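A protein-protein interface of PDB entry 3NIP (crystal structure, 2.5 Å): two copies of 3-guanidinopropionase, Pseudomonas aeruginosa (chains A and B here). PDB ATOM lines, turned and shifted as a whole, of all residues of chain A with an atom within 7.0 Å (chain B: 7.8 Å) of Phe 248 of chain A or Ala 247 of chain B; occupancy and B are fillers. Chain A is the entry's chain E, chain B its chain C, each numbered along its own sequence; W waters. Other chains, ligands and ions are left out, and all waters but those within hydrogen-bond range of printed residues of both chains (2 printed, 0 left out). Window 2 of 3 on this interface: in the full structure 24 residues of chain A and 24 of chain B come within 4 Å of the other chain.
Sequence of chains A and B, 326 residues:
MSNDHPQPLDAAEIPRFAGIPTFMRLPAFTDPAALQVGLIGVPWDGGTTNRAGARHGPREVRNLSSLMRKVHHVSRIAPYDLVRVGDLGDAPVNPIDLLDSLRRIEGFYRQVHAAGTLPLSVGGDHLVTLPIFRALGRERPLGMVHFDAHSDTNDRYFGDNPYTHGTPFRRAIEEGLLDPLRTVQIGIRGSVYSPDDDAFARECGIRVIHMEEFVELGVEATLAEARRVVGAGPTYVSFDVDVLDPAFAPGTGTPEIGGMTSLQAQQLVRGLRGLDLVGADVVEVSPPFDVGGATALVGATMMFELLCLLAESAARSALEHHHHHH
The side-chain carboxylate of Asp 245 of chain B sits at hydrogen-bond distance from the backbone NH of Ala 247 of chain B (2.9 Å). The side-chain carboxylate of Asp 245 of chain B lies within hydrogen-bond range of the backbone NH of Gly 258 of chain B, at 2.9 Å. The side-chain carboxylate of Asp 245 of chain B is in hydrogen-bond range of the backbone NH of Gly 259 of chain B, at 3.0 Å. The backbone carbonyl oxygen (O) of Met 260 of chain B is in hydrogen-bond range of the backbone NH (N) of Asp 245 of chain B, at 2.9 Å. N of Ala 247 of chain A sits close to OD2 of Asp 245 of chain A (3.1 Å). The side-chain hydroxyl (OG1) of Thr 261 of chain A sits close to the backbone NH (N) of Leu 263 of chain A (3.4 Å).
O of Ala 247 of chain A touches CB of Ala 247 of chain B (3.3 Å). CD1 of Phe 248 of chain A touches OD2 of Asp 245 of chain B (3.2 Å). Phe 248 of chain A touches Ala 247 of chain B (CD1 to CB, 3.6 Å). OD1 of Asp 245 of chain B touches CB of Ser 262 of chain A (3.8 Å). CB of Ser 262 of chain A touches N of Gly 258 of chain B, at 3.5 Å. Leu 263 of chain A touches Gly 258 of chain B (N to CA, 3.6 Å).
Phe 248 of chain A touches just these residues of chain B: Asp 245 (3.2 Å) and Ala 247 (3.6 Å). Of the printed residues of chain B, Ser 262 of chain A touches Asp 245 and Gly 258. Printed residues of chain A within 4 Å of Asp 245 of chain B: Phe 248 and Ser 262. Ala 247 of chain B touches just these residues of chain A: Ala 247 (3.3 Å) and Phe 248 (3.6 Å). Of the printed residues of chain A, Gly 258 of chain B touches Ser 262 (3.5 Å) and Leu 263 (3.6 Å). The nearest printed residue of chain B that does not touch Ser 262 of chain A is Ile 257 of chain B (4.1 Å).
Printed residues of chain B that touch a printed residue of chain A: Asp 245, Ala 247 and Gly 258. Hydrophobic or aromatic side chains of chain B within 4 Å of the printed part of chain A: Ala 247.
Ala 247 of chain B touches its own counterpart, Ala 247 of chain A. Phe 248 of chain A touches Asp 245 of chain B, but with the chains exchanged Asp 245 of chain A does not touch Phe 248 of chain B (8.9 Å). Phe 248 of chain A touches Ala 247 of chain B, but with the chains exchanged Ala 247 of chain A does not touch Phe 248 of chain B (5.9 Å). Ser 262 of chain A touches Asp 245 of chain B, but with the chains exchanged Asp 245 of chain A does not touch Ser 262 of chain B (13.3 Å).
Water W2 lies within hydrogen-bond range of the side-chain hydroxyl (OG) of Ser 262 of chain A (2.6 Å) and the side-chain carboxylate (OD2) of Asp 245 of chain B (2.7 Å). Water W1 lies within hydrogen-bond range of the backbone NH of Leu 263 of chain A, the side-chain carboxylate of Asp 245 of chain B and the backbone NH of Ser 262 of chain A.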
ATOM      1  N   VAL A 241      -8.095 -23.147   5.613  1.00  0.00           N
ATOM      2  CA  VAL A 241      -9.315 -23.149   4.796  1.00  0.00           C
ATOM      3  C   VAL A 241      -9.530 -24.463   4.060  1.00  0.00           C
ATOM      4  O   VAL A 241     -10.665 -24.801   3.733  1.00  0.00           O
ATOM      5  CB  VAL A 241      -9.400 -21.963   3.800  1.00  0.00           C
ATOM      6  CG1 VAL A 241      -9.581 -20.637   4.525  1.00  0.00           C
ATOM      7  CG2 VAL A 241      -8.191 -21.927   2.872  1.00  0.00           C
ATOM      8  N   LEU A 244     -12.375 -26.904   4.856  1.00  0.00           N
ATOM      9  CA  LEU A 244     -13.708 -26.766   4.267  1.00  0.00           C
ATOM     10  C   LEU A 244     -13.783 -27.550   2.978  1.00  0.00           C
ATOM     11  O   LEU A 244     -12.774 -27.750   2.325  1.00  0.00           O
ATOM     12  CB  LEU A 244     -14.028 -25.298   3.983  1.00  0.00           C
ATOM     13  CG  LEU A 244     -14.059 -24.393   5.209  1.00  0.00           C
ATOM     14  CD1 LEU A 244     -14.003 -22.953   4.755  1.00  0.00           C
ATOM     15  CD2 LEU A 244     -15.268 -24.651   6.110  1.00  0.00           C
ATOM     16  N   ASP A 245     -14.977 -27.998   2.611  1.00  0.00           N
ATOM     17  CA  ASP A 245     -15.152 -28.562   1.294  1.00  0.00           C
ATOM     18  C   ASP A 245     -14.740 -27.546   0.224  1.00  0.00           C
ATOM     19  O   ASP A 245     -14.938 -26.337   0.384  1.00  0.00           O
ATOM     20  CB  ASP A 245     -16.587 -29.071   1.067  1.00  0.00           C
ATOM     21  CG  ASP A 245     -16.657 -30.108  -0.059  1.00  0.00           C
ATOM     22  OD1 ASP A 245     -16.612 -31.316   0.258  1.00  0.00           O
ATOM     23  OD2 ASP A 245     -16.695 -29.722  -1.251  1.00  0.00           O
ATOM     24  N   PRO A 246     -14.131 -28.028  -0.861  1.00  0.00           N
ATOM     25  CA  PRO A 246     -13.810 -27.168  -2.008  1.00  0.00           C
ATOM     26  C   PRO A 246     -14.980 -26.336  -2.512  1.00  0.00           C
ATOM     27  O   PRO A 246     -14.769 -25.281  -3.101  1.00  0.00           O
ATOM     28  CB  PRO A 246     -13.406 -28.175  -3.061  1.00  0.00           C
ATOM     29  CG  PRO A 246     -12.725 -29.251  -2.269  1.00  0.00           C
ATOM     30  CD  PRO A 246     -13.464 -29.340  -0.960  1.00  0.00           C
ATOM     31  N   ALA A 247     -16.201 -26.809  -2.283  1.00  0.00           N
ATOM     32  CA  ALA A 247     -17.419 -26.067  -2.617  1.00  0.00           C
ATOM     33  C   ALA A 247     -17.477 -24.734  -1.896  1.00  0.00           C
ATOM     34  O   ALA A 247     -18.003 -23.751  -2.418  1.00  0.00           O
ATOM     35  CB  ALA A 247     -18.665 -26.902  -2.270  1.00  0.00           C
ATOM     36  N   PHE A 248     -16.947 -24.732  -0.680  1.00  0.00           N
ATOM     37  CA  PHE A 248     -16.925 -23.549   0.177  1.00  0.00           C
ATOM     38  C   PHE A 248     -15.593 -22.837   0.104  1.00  0.00           C
ATOM     39  O   PHE A 248     -15.550 -21.631   0.273  1.00  0.00           O
ATOM     40  CB  PHE A 248     -17.223 -23.937   1.621  1.00  0.00           C
ATOM     41  CG  PHE A 248     -18.497 -24.702   1.787  1.00  0.00           C
ATOM     42  CD1 PHE A 248     -19.725 -24.042   1.782  1.00  0.00           C
ATOM     43  CD2 PHE A 248     -18.476 -26.095   1.939  1.00  0.00           C
ATOM     44  CE1 PHE A 248     -20.923 -24.748   1.936  1.00  0.00           C
ATOM     45  CE2 PHE A 248     -19.669 -26.815   2.080  1.00  0.00           C
ATOM     46  CZ  PHE A 248     -20.895 -26.135   2.089  1.00  0.00           C
ATOM     47  N   ALA A 249     -14.510 -23.578  -0.145  1.00  0.00           N
ATOM     48  CA  ALA A 249     -13.168 -22.984  -0.257  1.00  0.00           C
ATOM     49  C   ALA A 249     -12.377 -23.466  -1.486  1.00  0.00           C
ATOM     50  O   ALA A 249     -11.411 -24.206  -1.352  1.00  0.00           O
ATOM     51  CB  ALA A 249     -12.362 -23.219   1.047  1.00  0.00           C
ATOM     52  N   PRO A 250     -12.767 -23.033  -2.696  1.00  0.00           N
ATOM     53  CA  PRO A 250     -12.026 -23.549  -3.868  1.00  0.00           C
ATOM     54  C   PRO A 250     -10.578 -23.030  -3.953  1.00  0.00           C
ATOM     55  O   PRO A 250      -9.700 -23.718  -4.469  1.00  0.00           O
ATOM     56  CB  PRO A 250     -12.854 -23.051  -5.059  1.00  0.00           C
ATOM     57  CG  PRO A 250     -13.573 -21.865  -4.560  1.00  0.00           C
ATOM     58  CD  PRO A 250     -13.815 -22.066  -3.080  1.00  0.00           C
ATOM     59  N   GLY A 251     -10.330 -21.836  -3.436  1.00  0.00           N
ATOM     60  CA  GLY A 251      -9.021 -21.202  -3.577  1.00  0.00           C
ATOM     61  C   GLY A 251      -8.040 -21.668  -2.523  1.00  0.00           C
ATOM     62  O   GLY A 251      -7.759 -20.939  -1.565  1.00  0.00           O
ATOM     63  N   GLY A 259     -15.478 -32.247   2.667  1.00  0.00           N
ATOM     64  CA  GLY A 259     -15.033 -31.510   3.837  1.00  0.00           C
ATOM     65  C   GLY A 259     -16.116 -30.821   4.637  1.00  0.00           C
ATOM     66  O   GLY A 259     -17.313 -30.953   4.351  1.00  0.00           O
ATOM     67  N   MET A 260     -15.668 -30.079   5.642  1.00  0.00           N
ATOM     68  CA  MET A 260     -16.527 -29.281   6.521  1.00  0.00           C
ATOM     69  C   MET A 260     -17.235 -28.177   5.737  1.00  0.00           C
ATOM     70  O   MET A 260     -16.737 -27.719   4.709  1.00  0.00           O
ATOM     71  CB  MET A 260     -15.643 -28.672   7.610  1.00  0.00           C
ATOM     72  CG  MET A 260     -16.356 -28.056   8.792  1.00  0.00           C
ATOM     73  SD  MET A 260     -15.196 -27.439  10.040  1.00  0.00           S
ATOM     74  CE  MET A 260     -14.543 -28.979  10.701  1.00  0.00           C
ATOM     75  N   THR A 261     -18.394 -27.748   6.218  1.00  0.00           N
ATOM     76  CA  THR A 261     -19.101 -26.636   5.603  1.00  0.00           C
ATOM     77  C   THR A 261     -18.719 -25.359   6.328  1.00  0.00           C
ATOM     78  O   THR A 261     -18.330 -25.404   7.501  1.00  0.00           O
ATOM     79  CB  THR A 261     -20.649 -26.804   5.677  1.00  0.00           C
ATOM     80  OG1 THR A 261     -21.098 -26.590   7.023  1.00  0.00           O
ATOM     81  CG2 THR A 261     -21.093 -28.189   5.182  1.00  0.00           C
ATOM     82  N   SER A 262     -18.841 -24.224   5.630  1.00  0.00           N
ATOM     83  CA  SER A 262     -18.724 -22.893   6.245  1.00  0.00           C
ATOM     84  C   SER A 262     -19.515 -22.809   7.549  1.00  0.00           C
ATOM     85  O   SER A 262     -19.005 -22.328   8.565  1.00  0.00           O
ATOM     86  CB  SER A 262     -19.221 -21.804   5.291  1.00  0.00           C
ATOM     87  OG  SER A 262     -18.314 -21.608   4.232  1.00  0.00           O
ATOM     88  N   LEU A 263     -20.757 -23.288   7.504  1.00  0.00           N
ATOM     89  CA  LEU A 263     -21.643 -23.279   8.655  1.00  0.00           C
ATOM     90  C   LEU A 263     -21.052 -24.030   9.855  1.00  0.00           C
ATOM     91  O   LEU A 263     -21.017 -23.498  10.975  1.00  0.00           O
ATOM     92  CB  LEU A 263     -22.995 -23.858   8.260  1.00  0.00           C
ATOM     93  CG  LEU A 263     -24.020 -24.092   9.367  1.00  0.00           C
ATOM     94  CD1 LEU A 263     -24.407 -22.777  10.040  1.00  0.00           C
ATOM     95  CD2 LEU A 263     -25.231 -24.769   8.773  1.00  0.00           C
ATOM     96  N   GLN A 264     -20.583 -25.258   9.616  1.00  0.00           N
ATOM     97  CA  GLN A 264     -19.987 -26.060  10.670  1.00  0.00           C
ATOM     98  C   GLN A 264     -18.774 -25.357  11.288  1.00  0.00           C
ATOM     99  O   GLN A 264     -18.664 -25.283  12.522  1.00  0.00           O
ATOM    100  CB  GLN A 264     -19.615 -27.448  10.150  1.00  0.00           C
ATOM    101  CG  GLN A 264     -20.814 -28.393   9.970  1.00  0.00           C
ATOM    102  CD  GLN A 264     -20.498 -29.637   9.124  1.00  0.00           C
ATOM    103  OE1 GLN A 264     -19.568 -29.646   8.301  1.00  0.00           O
ATOM    104  NE2 GLN A 264     -21.295 -30.683   9.311  1.00  0.00           N
ATOM    105  N   ASP A 290      -8.770 -19.274  -6.463  1.00  0.00           N
ATOM    106  CA  ASP A 290     -10.071 -18.862  -5.907  1.00  0.00           C
ATOM    107  C   ASP A 290     -11.042 -18.573  -7.049  1.00  0.00           C
ATOM    108  O   ASP A 290     -10.641 -18.459  -8.193  1.00  0.00           O
ATOM    109  CB  ASP A 290      -9.906 -17.636  -4.996  1.00  0.00           C
ATOM    110  CG  ASP A 290     -10.984 -17.534  -3.906  1.00  0.00           C
ATOM    111  OD1 ASP A 290     -11.905 -18.380  -3.824  1.00  0.00           O
ATOM    112  OD2 ASP A 290     -10.912 -16.578  -3.103  1.00  0.00           O
ATOM    113  N   ALA A 294     -14.397 -16.166  -3.420  1.00  0.00           N
ATOM    114  CA  ALA A 294     -15.131 -16.968  -2.433  1.00  0.00           C
ATOM    115  C   ALA A 294     -14.295 -17.278  -1.181  1.00  0.00           C
ATOM    116  O   ALA A 294     -14.745 -17.056  -0.052  1.00  0.00           O
ATOM    117  CB  ALA A 294     -15.660 -18.268  -3.064  1.00  0.00           C
ATOM    118  N   THR A 295     -13.079 -17.783  -1.386  1.00  0.00           N
ATOM    119  CA  THR A 295     -12.262 -18.255  -0.276  1.00  0.00           C
ATOM    120  C   THR A 295     -11.683 -17.091   0.516  1.00  0.00           C
ATOM    121  O   THR A 295     -11.520 -17.194   1.737  1.00  0.00           O
ATOM    122  CB  THR A 295     -11.122 -19.160  -0.757  1.00  0.00           C
ATOM    123  OG1 THR A 295     -11.608 -20.001  -1.806  1.00  0.00           O
ATOM    124  CG2 THR A 295     -10.564 -20.015   0.408  1.00  0.00           C
ATOM    125  N   VAL A 298     -14.470 -16.234   2.823  1.00  0.00           N
ATOM    126  CA  VAL A 298     -14.433 -17.202   3.910  1.00  0.00           C
ATOM    127  C   VAL A 298     -13.319 -16.832   4.892  1.00  0.00           C
ATOM    128  O   VAL A 298     -13.542 -16.759   6.100  1.00  0.00           O
ATOM    129  CB  VAL A 298     -14.209 -18.637   3.376  1.00  0.00           C
ATOM    130  CG1 VAL A 298     -13.869 -19.567   4.512  1.00  0.00           C
ATOM    131  CG2 VAL A 298     -15.444 -19.122   2.626  1.00  0.00           C
ATOM    132  N   LEU B 244     -29.055 -18.555   0.613  1.00  0.00           N
ATOM    133  CA  LEU B 244     -28.230 -19.712   0.326  1.00  0.00           C
ATOM    134  C   LEU B 244     -26.756 -19.421   0.590  1.00  0.00           C
ATOM    135  O   LEU B 244     -26.274 -18.291   0.393  1.00  0.00           O
ATOM    136  CB  LEU B 244     -28.402 -20.130  -1.141  1.00  0.00           C
ATOM    137  CG  LEU B 244     -29.780 -20.613  -1.605  1.00  0.00           C
ATOM    138  CD1 LEU B 244     -29.839 -20.741  -3.117  1.00  0.00           C
ATOM    139  CD2 LEU B 244     -30.129 -21.937  -0.967  1.00  0.00           C
ATOM    140  N   ASP B 245     -26.040 -20.453   1.028  1.00  0.00           N
ATOM    141  CA  ASP B 245     -24.598 -20.363   1.133  1.00  0.00           C
ATOM    142  C   ASP B 245     -24.033 -19.957  -0.219  1.00  0.00           C
ATOM    143  O   ASP B 245     -24.527 -20.404  -1.255  1.00  0.00           O
ATOM    144  CB  ASP B 245     -23.996 -21.701   1.579  1.00  0.00           C
ATOM    145  CG  ASP B 245     -22.559 -21.559   2.052  1.00  0.00           C
ATOM    146  OD1 ASP B 245     -22.370 -21.378   3.281  1.00  0.00           O
ATOM    147  OD2 ASP B 245     -21.635 -21.585   1.195  1.00  0.00           O
ATOM    148  N   PRO B 246     -23.003 -19.092  -0.219  1.00  0.00           N
ATOM    149  CA  PRO B 246     -22.245 -18.743  -1.436  1.00  0.00           C
ATOM    150  C   PRO B 246     -21.864 -19.942  -2.318  1.00  0.00           C
ATOM    151  O   PRO B 246     -21.778 -19.806  -3.536  1.00  0.00           O
ATOM    152  CB  PRO B 246     -21.002 -18.085  -0.869  1.00  0.00           C
ATOM    153  CG  PRO B 246     -21.540 -17.338   0.356  1.00  0.00           C
ATOM    154  CD  PRO B 246     -22.610 -18.253   0.934  1.00  0.00           C
ATOM    155  N   ALA B 247     -21.654 -21.109  -1.707  1.00  0.00           N
ATOM    156  CA  ALA B 247     -21.367 -22.337  -2.446  1.00  0.00           C
ATOM    157  C   ALA B 247     -22.469 -22.710  -3.440  1.00  0.00           C
ATOM    158  O   ALA B 247     -22.181 -23.233  -4.528  1.00  0.00           O
ATOM    159  CB  ALA B 247     -21.131 -23.474  -1.495  1.00  0.00           C
ATOM    160  N   PHE B 248     -23.718 -22.444  -3.051  1.00  0.00           N
ATOM    161  CA  PHE B 248     -24.869 -22.741  -3.879  1.00  0.00           C
ATOM    162  C   PHE B 248     -25.274 -21.532  -4.705  1.00  0.00           C
ATOM    163  O   PHE B 248     -25.809 -21.687  -5.797  1.00  0.00           O
ATOM    164  CB  PHE B 248     -26.032 -23.226  -3.019  1.00  0.00           C
ATOM    165  CG  PHE B 248     -25.689 -24.406  -2.164  1.00  0.00           C
ATOM    166  CD1 PHE B 248     -25.662 -25.698  -2.710  1.00  0.00           C
ATOM    167  CD2 PHE B 248     -25.374 -24.234  -0.819  1.00  0.00           C
ATOM    168  CE1 PHE B 248     -25.331 -26.806  -1.926  1.00  0.00           C
ATOM    169  CE2 PHE B 248     -25.037 -25.328  -0.022  1.00  0.00           C
ATOM    170  CZ  PHE B 248     -25.015 -26.626  -0.579  1.00  0.00           C
ATOM    171  N   ALA B 249     -25.015 -20.336  -4.196  1.00  0.00           N
ATOM    172  CA  ALA B 249     -25.369 -19.110  -4.899  1.00  0.00           C
ATOM    173  C   ALA B 249     -24.249 -18.060  -4.850  1.00  0.00           C
ATOM    174  O   ALA B 249     -24.352 -17.079  -4.122  1.00  0.00           O
ATOM    175  CB  ALA B 249     -26.681 -18.532  -4.332  1.00  0.00           C
ATOM    176  N   PRO B 250     -23.182 -18.246  -5.626  1.00  0.00           N
ATOM    177  CA  PRO B 250     -22.114 -17.237  -5.581  1.00  0.00           C
ATOM    178  C   PRO B 250     -22.485 -15.882  -6.201  1.00  0.00           C
ATOM    179  O   PRO B 250     -21.908 -14.862  -5.838  1.00  0.00           O
ATOM    180  CB  PRO B 250     -20.989 -17.880  -6.403  1.00  0.00           C
ATOM    181  CG  PRO B 250     -21.695 -18.844  -7.341  1.00  0.00           C
ATOM    182  CD  PRO B 250     -22.896 -19.341  -6.579  1.00  0.00           C
ATOM    183  N   GLY B 251     -23.440 -15.879  -7.131  1.00  0.00           N
ATOM    184  CA  GLY B 251     -23.748 -14.704  -7.945  1.00  0.00           C
ATOM    185  C   GLY B 251     -24.763 -13.822  -7.263  1.00  0.00           C
ATOM    186  O   GLY B 251     -25.917 -13.720  -7.696  1.00  0.00           O
ATOM    187  N   GLU B 256     -23.289 -13.862   2.672  1.00  0.00           N
ATOM    188  CA  GLU B 256     -22.921 -14.124   4.043  1.00  0.00           C
ATOM    189  C   GLU B 256     -22.719 -15.616   4.074  1.00  0.00           C
ATOM    190  O   GLU B 256     -23.644 -16.369   3.730  1.00  0.00           O
ATOM    191  CB  GLU B 256     -24.039 -13.736   5.030  1.00  0.00           C
ATOM    192  CG  GLU B 256     -24.623 -12.330   4.859  1.00  0.00           C
ATOM    193  CD  GLU B 256     -23.678 -11.203   5.270  1.00  0.00           C
ATOM    194  OE1 GLU B 256     -22.660 -11.451   5.953  1.00  0.00           O
ATOM    195  OE2 GLU B 256     -23.971 -10.046   4.916  1.00  0.00           O
ATOM    196  N   ILE B 257     -21.528 -16.060   4.470  1.00  0.00           N
ATOM    197  CA  ILE B 257     -21.230 -17.498   4.478  1.00  0.00           C
ATOM    198  C   ILE B 257     -22.067 -18.266   5.510  1.00  0.00           C
ATOM    199  O   ILE B 257     -22.809 -17.665   6.301  1.00  0.00           O
ATOM    200  CB  ILE B 257     -19.717 -17.793   4.669  1.00  0.00           C
ATOM    201  CG1 ILE B 257     -19.257 -17.468   6.101  1.00  0.00           C
ATOM    202  CG2 ILE B 257     -18.872 -17.102   3.577  1.00  0.00           C
ATOM    203  CD1 ILE B 257     -17.879 -17.989   6.437  1.00  0.00           C
ATOM    204  N   GLY B 258     -21.951 -19.594   5.487  1.00  0.00           N
ATOM    205  CA  GLY B 258     -22.652 -20.461   6.440  1.00  0.00           C
ATOM    206  C   GLY B 258     -24.157 -20.409   6.269  1.00  0.00           C
ATOM    207  O   GLY B 258     -24.901 -20.257   7.244  1.00  0.00           O
ATOM    208  N   GLY B 259     -24.611 -20.544   5.027  1.00  0.00           N
ATOM    209  CA  GLY B 259     -26.036 -20.465   4.736  1.00  0.00           C
ATOM    210  C   GLY B 259     -26.769 -21.774   4.490  1.00  0.00           C
ATOM    211  O   GLY B 259     -26.253 -22.876   4.697  1.00  0.00           O
ATOM    212  N   MET B 260     -27.998 -21.616   4.026  1.00  0.00           N
ATOM    213  CA  MET B 260     -28.894 -22.693   3.701  1.00  0.00           C
ATOM    214  C   MET B 260     -28.410 -23.360   2.402  1.00  0.00           C
ATOM    215  O   MET B 260     -27.772 -22.716   1.563  1.00  0.00           O
ATOM    216  CB  MET B 260     -30.268 -22.044   3.535  1.00  0.00           C
ATOM    217  CG  MET B 260     -31.447 -22.942   3.350  1.00  0.00           C
ATOM    218  SD  MET B 260     -33.005 -22.003   3.226  1.00  0.00           S
ATOM    219  CE  MET B 260     -33.103 -21.320   4.896  1.00  0.00           C
ATOM    220  N   THR B 261     -28.688 -24.651   2.257  1.00  0.00           N
ATOM    221  CA  THR B 261     -28.386 -25.387   1.026  1.00  0.00           C
ATOM    222  C   THR B 261     -29.566 -25.315   0.065  1.00  0.00           C
ATOM    223  O   THR B 261     -30.703 -25.088   0.501  1.00  0.00           O
ATOM    224  CB  THR B 261     -28.108 -26.877   1.320  1.00  0.00           C
ATOM    225  OG1 THR B 261     -29.338 -27.530   1.672  1.00  0.00           O
ATOM    226  CG2 THR B 261     -27.088 -27.021   2.456  1.00  0.00           C
ATOM    227  N   SER B 262     -29.307 -25.515  -1.232  1.00  0.00           N
ATOM    228  CA  SER B 262     -30.385 -25.603  -2.242  1.00  0.00           C
ATOM    229  C   SER B 262     -31.441 -26.593  -1.820  1.00  0.00           C
ATOM    230  O   SER B 262     -32.642 -26.283  -1.862  1.00  0.00           O
ATOM    231  CB  SER B 262     -29.856 -26.017  -3.603  1.00  0.00           C
ATOM    232  OG  SER B 262     -28.948 -25.057  -4.072  1.00  0.00           O
ATOM    233  N   ALA B 294     -24.495 -20.607 -12.314  1.00  0.00           N
ATOM    234  CA  ALA B 294     -24.951 -21.334 -11.133  1.00  0.00           C
ATOM    235  C   ALA B 294     -26.125 -20.635 -10.437  1.00  0.00           C
ATOM    236  O   ALA B 294     -27.168 -21.249 -10.164  1.00  0.00           O
ATOM    237  CB  ALA B 294     -23.798 -21.553 -10.152  1.00  0.00           C
ATOM    238  N   THR B 295     -25.971 -19.342 -10.174  1.00  0.00           N
ATOM    239  CA  THR B 295     -27.009 -18.632  -9.432  1.00  0.00           C
ATOM    240  C   THR B 295     -28.271 -18.421 -10.299  1.00  0.00           C
ATOM    241  O   THR B 295     -29.400 -18.564  -9.813  1.00  0.00           O
ATOM    242  CB  THR B 295     -26.455 -17.342  -8.812  1.00  0.00           C
ATOM    243  OG1 THR B 295     -25.148 -17.618  -8.272  1.00  0.00           O
ATOM    244  CG2 THR B 295     -27.354 -16.863  -7.700  1.00  0.00           C
ATOM    245  N   VAL B 298     -30.170 -21.848  -9.973  1.00  0.00           N
ATOM    246  CA  VAL B 298     -30.852 -21.828  -8.700  1.00  0.00           C
ATOM    247  C   VAL B 298     -32.104 -20.942  -8.772  1.00  0.00           C
ATOM    248  O   VAL B 298     -33.194 -21.361  -8.348  1.00  0.00           O
ATOM    249  CB  VAL B 298     -29.910 -21.348  -7.586  1.00  0.00           C
ATOM    250  CG1 VAL B 298     -30.696 -20.823  -6.386  1.00  0.00           C
ATOM    251  CG2 VAL B 298     -28.996 -22.480  -7.169  1.00  0.00           C
HETATM  252  O   HOH W   1     -21.876 -23.737   4.934  1.00  0.00           O
HETATM  253  O   HOH W   2     -19.433 -20.399   2.205  1.00  0.00           O
